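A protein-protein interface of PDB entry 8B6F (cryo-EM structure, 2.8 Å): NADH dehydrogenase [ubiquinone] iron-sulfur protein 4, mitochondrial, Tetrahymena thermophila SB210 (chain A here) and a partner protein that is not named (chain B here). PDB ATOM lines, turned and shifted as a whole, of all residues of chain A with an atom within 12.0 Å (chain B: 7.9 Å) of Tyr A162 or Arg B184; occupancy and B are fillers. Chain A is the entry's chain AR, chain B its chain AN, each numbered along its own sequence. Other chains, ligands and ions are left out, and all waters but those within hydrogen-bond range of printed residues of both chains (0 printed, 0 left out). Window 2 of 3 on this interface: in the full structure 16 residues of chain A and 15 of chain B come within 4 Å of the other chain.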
ATOM      1  N   GLY A  51     -28.331  -6.711  35.228  1.00  0.00           N
ATOM      2  CA  GLY A  51     -28.014  -7.172  36.561  1.00  0.00           C
ATOM      3  C   GLY A  51     -27.219  -8.464  36.547  1.00  0.00           C
ATOM      4  O   GLY A  51     -27.169  -9.192  35.556  1.00  0.00           O
ATOM      5  N   GLN A  52     -26.575  -8.744  37.681  1.00  0.00           N
ATOM      6  CA  GLN A  52     -25.704  -9.904  37.802  1.00  0.00           C
ATOM      7  C   GLN A  52     -25.923 -10.719  39.067  1.00  0.00           C
ATOM      8  O   GLN A  52     -25.338 -11.802  39.180  1.00  0.00           O
ATOM      9  CB  GLN A  52     -24.232  -9.468  37.750  1.00  0.00           C
ATOM     10  CG  GLN A  52     -23.866  -8.701  36.489  1.00  0.00           C
ATOM     11  CD  GLN A  52     -22.433  -8.213  36.502  1.00  0.00           C
ATOM     12  OE1 GLN A  52     -21.681  -8.488  37.436  1.00  0.00           O
ATOM     13  NE2 GLN A  52     -22.048  -7.481  35.463  1.00  0.00           N
ATOM     14  N   ASP A  89     -30.696 -21.317  26.933  1.00  0.00           N
ATOM     15  CA  ASP A  89     -29.780 -21.344  25.806  1.00  0.00           C
ATOM     16  C   ASP A  89     -29.842 -22.694  25.100  1.00  0.00           C
ATOM     17  O   ASP A  89     -30.398 -23.670  25.607  1.00  0.00           O
ATOM     18  CB  ASP A  89     -28.352 -21.059  26.273  1.00  0.00           C
ATOM     19  CG  ASP A  89     -28.203 -19.680  26.882  1.00  0.00           C
ATOM     20  OD1 ASP A  89     -28.851 -18.736  26.386  1.00  0.00           O
ATOM     21  OD2 ASP A  89     -27.438 -19.541  27.862  1.00  0.00           O
ATOM     22  N   PHE A 157     -29.780 -14.542  36.136  1.00  0.00           N
ATOM     23  CA  PHE A 157     -29.310 -13.842  34.953  1.00  0.00           C
ATOM     24  C   PHE A 157     -28.412 -14.740  34.104  1.00  0.00           C
ATOM     25  O   PHE A 157     -27.759 -15.649  34.621  1.00  0.00           O
ATOM     26  CB  PHE A 157     -28.567 -12.578  35.354  1.00  0.00           C
ATOM     27  CG  PHE A 157     -29.431 -11.583  36.068  1.00  0.00           C
ATOM     28  CD1 PHE A 157     -29.554 -11.615  37.444  1.00  0.00           C
ATOM     29  CD2 PHE A 157     -30.138 -10.629  35.357  1.00  0.00           C
ATOM     30  CE1 PHE A 157     -30.356 -10.703  38.100  1.00  0.00           C
ATOM     31  CE2 PHE A 157     -30.940  -9.716  36.006  1.00  0.00           C
ATOM     32  CZ  PHE A 157     -31.050  -9.753  37.380  1.00  0.00           C
ATOM     33  N   PRO A 158     -28.363 -14.500  32.795  1.00  0.00           N
ATOM     34  CA  PRO A 158     -27.643 -15.411  31.902  1.00  0.00           C
ATOM     35  C   PRO A 158     -26.135 -15.266  32.013  1.00  0.00           C
ATOM     36  O   PRO A 158     -25.604 -14.256  32.480  1.00  0.00           O
ATOM     37  CB  PRO A 158     -28.125 -14.991  30.511  1.00  0.00           C
ATOM     38  CG  PRO A 158     -28.424 -13.541  30.665  1.00  0.00           C
ATOM     39  CD  PRO A 158     -28.966 -13.375  32.057  1.00  0.00           C
ATOM     40  N   ARG A 159     -25.445 -16.312  31.566  1.00  0.00           N
ATOM     41  CA  ARG A 159     -23.996 -16.315  31.437  1.00  0.00           C
ATOM     42  C   ARG A 159     -23.637 -16.736  30.020  1.00  0.00           C
ATOM     43  O   ARG A 159     -24.242 -17.658  29.467  1.00  0.00           O
ATOM     44  CB  ARG A 159     -23.343 -17.259  32.455  1.00  0.00           C
ATOM     45  CG  ARG A 159     -23.609 -16.889  33.908  1.00  0.00           C
ATOM     46  CD  ARG A 159     -23.094 -15.492  34.231  1.00  0.00           C
ATOM     47  NE  ARG A 159     -23.302 -15.135  35.630  1.00  0.00           N
ATOM     48  CZ  ARG A 159     -22.414 -15.316  36.598  1.00  0.00           C
ATOM     49  NH1 ARG A 159     -21.232 -15.858  36.361  1.00  0.00           N
ATOM     50  NH2 ARG A 159     -22.720 -14.939  37.835  1.00  0.00           N
ATOM     51  N   SER A 160     -22.655 -16.056  29.435  1.00  0.00           N
ATOM     52  CA  SER A 160     -22.273 -16.273  28.047  1.00  0.00           C
ATOM     53  C   SER A 160     -20.760 -16.397  27.943  1.00  0.00           C
ATOM     54  O   SER A 160     -20.018 -16.087  28.879  1.00  0.00           O
ATOM     55  CB  SER A 160     -22.781 -15.140  27.145  1.00  0.00           C
ATOM     56  OG  SER A 160     -22.324 -13.879  27.601  1.00  0.00           O
ATOM     57  N   ARG A 161     -20.306 -16.859  26.782  1.00  0.00           N
ATOM     58  CA  ARG A 161     -18.883 -17.057  26.553  1.00  0.00           C
ATOM     59  C   ARG A 161     -18.148 -15.723  26.549  1.00  0.00           C
ATOM     60  O   ARG A 161     -18.642 -14.724  26.018  1.00  0.00           O
ATOM     61  CB  ARG A 161     -18.652 -17.770  25.222  1.00  0.00           C
ATOM     62  CG  ARG A 161     -19.395 -19.084  25.077  1.00  0.00           C
ATOM     63  CD  ARG A 161     -19.277 -19.622  23.660  1.00  0.00           C
ATOM     64  NE  ARG A 161     -19.989 -20.885  23.493  1.00  0.00           N
ATOM     65  CZ  ARG A 161     -19.448 -22.086  23.653  1.00  0.00           C
ATOM     66  NH1 ARG A 161     -18.179 -22.235  23.995  1.00  0.00           N
ATOM     67  NH2 ARG A 161     -20.202 -23.165  23.466  1.00  0.00           N
ATOM     68  N   TYR A 162     -16.958 -15.712  27.143  1.00  0.00           N
ATOM     69  CA  TYR A 162     -16.084 -14.550  27.060  1.00  0.00           C
ATOM     70  C   TYR A 162     -15.426 -14.514  25.689  1.00  0.00           C
ATOM     71  O   TYR A 162     -14.856 -15.511  25.239  1.00  0.00           O
ATOM     72  CB  TYR A 162     -15.012 -14.597  28.150  1.00  0.00           C
ATOM     73  CG  TYR A 162     -15.536 -14.516  29.567  1.00  0.00           C
ATOM     74  CD1 TYR A 162     -16.800 -14.011  29.841  1.00  0.00           C
ATOM     75  CD2 TYR A 162     -14.755 -14.940  30.633  1.00  0.00           C
ATOM     76  CE1 TYR A 162     -17.271 -13.935  31.137  1.00  0.00           C
ATOM     77  CE2 TYR A 162     -15.216 -14.870  31.930  1.00  0.00           C
ATOM     78  CZ  TYR A 162     -16.475 -14.367  32.176  1.00  0.00           C
ATOM     79  OH  TYR A 162     -16.937 -14.296  33.469  1.00  0.00           O
ATOM     80  N   HIS A 163     -15.511 -13.366  25.023  1.00  0.00           N
ATOM     81  CA  HIS A 163     -14.886 -13.226  23.716  1.00  0.00           C
ATOM     82  C   HIS A 163     -13.376 -13.375  23.839  1.00  0.00           C
ATOM     83  O   HIS A 163     -12.748 -12.771  24.714  1.00  0.00           O
ATOM     84  CB  HIS A 163     -15.237 -11.871  23.104  1.00  0.00           C
ATOM     85  CG  HIS A 163     -14.628 -11.647  21.755  1.00  0.00           C
ATOM     86  ND1 HIS A 163     -13.357 -11.138  21.588  1.00  0.00           N
ATOM     87  CD2 HIS A 163     -15.113 -11.865  20.511  1.00  0.00           C
ATOM     88  CE1 HIS A 163     -13.088 -11.052  20.297  1.00  0.00           C
ATOM     89  NE2 HIS A 163     -14.136 -11.487  19.622  1.00  0.00           N
ATOM     90  N   THR A 164     -12.794 -14.181  22.955  1.00  0.00           N
ATOM     91  CA  THR A 164     -11.359 -14.417  22.929  1.00  0.00           C
ATOM     92  C   THR A 164     -10.848 -14.258  21.506  1.00  0.00           C
ATOM     93  O   THR A 164     -11.560 -14.538  20.538  1.00  0.00           O
ATOM     94  CB  THR A 164     -11.002 -15.815  23.451  1.00  0.00           C
ATOM     95  OG1 THR A 164     -11.722 -16.807  22.709  1.00  0.00           O
ATOM     96  CG2 THR A 164     -11.340 -15.935  24.928  1.00  0.00           C
ATOM     97  N   ARG A 165      -9.604 -13.806  21.389  1.00  0.00           N
ATOM     98  CA  ARG A 165      -9.006 -13.602  20.078  1.00  0.00           C
ATOM     99  C   ARG A 165      -8.835 -14.940  19.374  1.00  0.00           C
ATOM    100  O   ARG A 165      -8.322 -15.900  19.955  1.00  0.00           O
ATOM    101  CB  ARG A 165      -7.662 -12.888  20.213  1.00  0.00           C
ATOM    102  CG  ARG A 165      -7.040 -12.499  18.882  1.00  0.00           C
ATOM    103  CD  ARG A 165      -5.920 -11.490  19.073  1.00  0.00           C
ATOM    104  NE  ARG A 165      -5.365 -11.044  17.802  1.00  0.00           N
ATOM    105  CZ  ARG A 165      -4.474 -10.068  17.675  1.00  0.00           C
ATOM    106  NH1 ARG A 165      -4.021  -9.404  18.725  1.00  0.00           N
ATOM    107  NH2 ARG A 165      -4.028  -9.752  16.463  1.00  0.00           N
ATOM    108  N   LYS A 166      -9.268 -14.999  18.117  1.00  0.00           N
ATOM    109  CA  LYS A 166      -9.254 -16.224  17.328  1.00  0.00           C
ATOM    110  C   LYS A 166      -8.523 -15.955  16.024  1.00  0.00           C
ATOM    111  O   LYS A 166      -8.805 -14.962  15.347  1.00  0.00           O
ATOM    112  CB  LYS A 166     -10.680 -16.710  17.050  1.00  0.00           C
ATOM    113  CG  LYS A 166     -10.827 -18.219  17.007  1.00  0.00           C
ATOM    114  CD  LYS A 166     -10.729 -18.823  18.401  1.00  0.00           C
ATOM    115  CE  LYS A 166     -10.999 -20.318  18.373  1.00  0.00           C
ATOM    116  NZ  LYS A 166     -10.899 -20.922  19.729  1.00  0.00           N
ATOM    117  N   ARG B 181     -21.236  -8.874  22.871  1.00  0.00           N
ATOM    118  CA  ARG B 181     -19.917  -9.286  23.325  1.00  0.00           C
ATOM    119  C   ARG B 181     -19.770  -9.053  24.823  1.00  0.00           C
ATOM    120  O   ARG B 181     -20.230  -8.042  25.360  1.00  0.00           O
ATOM    121  CB  ARG B 181     -18.833  -8.519  22.571  1.00  0.00           C
ATOM    122  CG  ARG B 181     -17.419  -8.807  23.055  1.00  0.00           C
ATOM    123  CD  ARG B 181     -16.394  -7.962  22.319  1.00  0.00           C
ATOM    124  NE  ARG B 181     -15.051  -8.162  22.850  1.00  0.00           N
ATOM    125  CZ  ARG B 181     -13.965  -7.561  22.388  1.00  0.00           C
ATOM    126  NH1 ARG B 181     -14.021  -6.717  21.371  1.00  0.00           N
ATOM    127  NH2 ARG B 181     -12.791  -7.811  22.961  1.00  0.00           N
ATOM    128  N   VAL B 182     -19.125 -10.001  25.495  1.00  0.00           N
ATOM    129  CA  VAL B 182     -18.775  -9.879  26.904  1.00  0.00           C
ATOM    130  C   VAL B 182     -17.306 -10.247  27.053  1.00  0.00           C
ATOM    131  O   VAL B 182     -16.883 -11.323  26.618  1.00  0.00           O
ATOM    132  CB  VAL B 182     -19.668 -10.764  27.798  1.00  0.00           C
ATOM    133  CG1 VAL B 182     -19.504 -12.239  27.459  1.00  0.00           C
ATOM    134  CG2 VAL B 182     -19.363 -10.514  29.269  1.00  0.00           C
ATOM    135  N   ASP B 183     -16.529  -9.345  27.641  1.00  0.00           N
ATOM    136  CA  ASP B 183     -15.107  -9.572  27.833  1.00  0.00           C
ATOM    137  C   ASP B 183     -14.848 -10.177  29.206  1.00  0.00           C
ATOM    138  O   ASP B 183     -15.609  -9.964  30.153  1.00  0.00           O
ATOM    139  CB  ASP B 183     -14.327  -8.264  27.690  1.00  0.00           C
ATOM    140  CG  ASP B 183     -14.532  -7.607  26.340  1.00  0.00           C
ATOM    141  OD1 ASP B 183     -14.707  -8.335  25.342  1.00  0.00           O
ATOM    142  OD2 ASP B 183     -14.522  -6.360  26.277  1.00  0.00           O
ATOM    143  N   ARG B 184     -13.767 -10.932  29.303  1.00  0.00           N
ATOM    144  CA  ARG B 184     -13.393 -11.532  30.575  1.00  0.00           C
ATOM    145  C   ARG B 184     -13.019 -10.431  31.558  1.00  0.00           C
ATOM    146  O   ARG B 184     -12.115  -9.638  31.266  1.00  0.00           O
ATOM    147  CB  ARG B 184     -12.225 -12.494  30.385  1.00  0.00           C
ATOM    148  CG  ARG B 184     -11.801 -13.206  31.659  1.00  0.00           C
ATOM    149  CD  ARG B 184     -10.593 -14.093  31.421  1.00  0.00           C
ATOM    150  NE  ARG B 184     -10.187 -14.783  32.640  1.00  0.00           N
ATOM    151  CZ  ARG B 184      -9.427 -14.251  33.588  1.00  0.00           C
ATOM    152  NH1 ARG B 184      -8.969 -13.013  33.495  1.00  0.00           N
ATOM    153  NH2 ARG B 184      -9.121 -14.979  34.658  1.00  0.00           N
ATOM    154  N   PRO B 185     -13.667 -10.336  32.718  1.00  0.00           N
ATOM    155  CA  PRO B 185     -13.311  -9.274  33.664  1.00  0.00           C
ATOM    156  C   PRO B 185     -11.917  -9.476  34.234  1.00  0.00           C
ATOM    157  O   PRO B 185     -11.424 -10.600  34.356  1.00  0.00           O
ATOM    158  CB  PRO B 185     -14.383  -9.391  34.753  1.00  0.00           C
ATOM    159  CG  PRO B 185     -14.832 -10.800  34.685  1.00  0.00           C
ATOM    160  CD  PRO B 185     -14.743 -11.195  33.240  1.00  0.00           C
ATOM    161  N   ALA B 186     -11.281  -8.361  34.580  1.00  0.00           N
ATOM    162  CA  ALA B 186      -9.968  -8.410  35.200  1.00  0.00           C
ATOM    163  C   ALA B 186     -10.072  -8.949  36.624  1.00  0.00           C
ATOM    164  O   ALA B 186     -11.146  -8.971  37.233  1.00  0.00           O
ATOM    165  CB  ALA B 186      -9.328  -7.023  35.211  1.00  0.00           C
ATOM    166  N   ARG B 187      -8.935  -9.392  37.152  1.00  0.00           N
ATOM    167  CA  ARG B 187      -8.910  -9.931  38.504  1.00  0.00           C
ATOM    168  C   ARG B 187      -9.433  -8.899  39.494  1.00  0.00           C
ATOM    169  O   ARG B 187      -9.083  -7.717  39.429  1.00  0.00           O
ATOM    170  CB  ARG B 187      -7.491 -10.353  38.884  1.00  0.00           C
ATOM    171  CG  ARG B 187      -7.384 -10.937  40.284  1.00  0.00           C
ATOM    172  CD  ARG B 187      -5.968 -11.383  40.601  1.00  0.00           C
ATOM    173  NE  ARG B 187      -5.027 -10.268  40.625  1.00  0.00           N
ATOM    174  CZ  ARG B 187      -4.830  -9.474  41.668  1.00  0.00           C
ATOM    175  NH1 ARG B 187      -5.513  -9.623  42.792  1.00  0.00           N
ATOM    176  NH2 ARG B 187      -3.922  -8.505  41.583  1.00  0.00           N
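Ser A160 touches Val B182 (OG to CG1, 3.3 Å). Arg A161 touches Val B182 (O to CG1, 3.0 Å). Tyr A162 touches Val B182 (CA to O, 3.4 Å). CB of Arg B184 touches CD2 of Tyr A162, 3.5 Å away. Pro B185 touches Tyr A162. His A163 touches Arg B181.
The backbone carbonyl oxygen (O) of Val B182 sits at hydrogen-bond distance from the backbone NH (N) of His A163.
Of the 7 printed residues of chain B, 4 touch a printed residue of chain A. Hydrophobic or aromatic side chains of chain B within 4 Å of the printed part of chain A: Val B182 and Pro B185. Of the 13 printed residues of chain A, 4 touch a printed residue of chain B. Hydrophobic or aromatic side chains of chain A within 4 Å of the printed part of chain B: Tyr A162 and His A163. Along chain A the printed residues that touch a printed residue of chain B span positions 160 to 163. Among the printed residues, 7 pairs touch across the chains. Among the printed residues, no Asp or Glu carboxylate lies within 4 Å of a Lys or Arg side-chain nitrogen of the other chain.
Arg B184 touches just one residue of chain A: Tyr A162. Of chain A, only Ser A160 (3.3 Å), Arg A161 (3.0 Å), Tyr A162 (3.4 Å) and His A163 (2.9 Å) come within 4 Å of Val B182. No residue of chain A comes within 4 Å of Asp B183. Of chain A, only Tyr A162 (3.8 Å) comes within 4 Å of Pro B185. Of the printed residues of chain B, Ser A160 touches Val B182. Printed residues of chain B within 4 Å of His A163: Arg B181 (3.6 Å) and Val B182 (2.9 Å). Of the printed residues of chain B, Arg A161 touches Val B182. Of the printed residues of chain A, Arg B181 touches His A163 (3.6 Å). Arg A165 touches none of the printed residues of chain B. Phe A157 touches none of the printed residues of chain B. The nearest residue of chain B that does not touch Tyr A162 is Asp B183 (4.2 Å). The nearest printed residue of chain B that does not touch Ser A160 is Arg B181 (6.1 Å).
OD1 of Asp B183 lies within salt-bridge range of NE of Arg B181 (2.5 Å).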
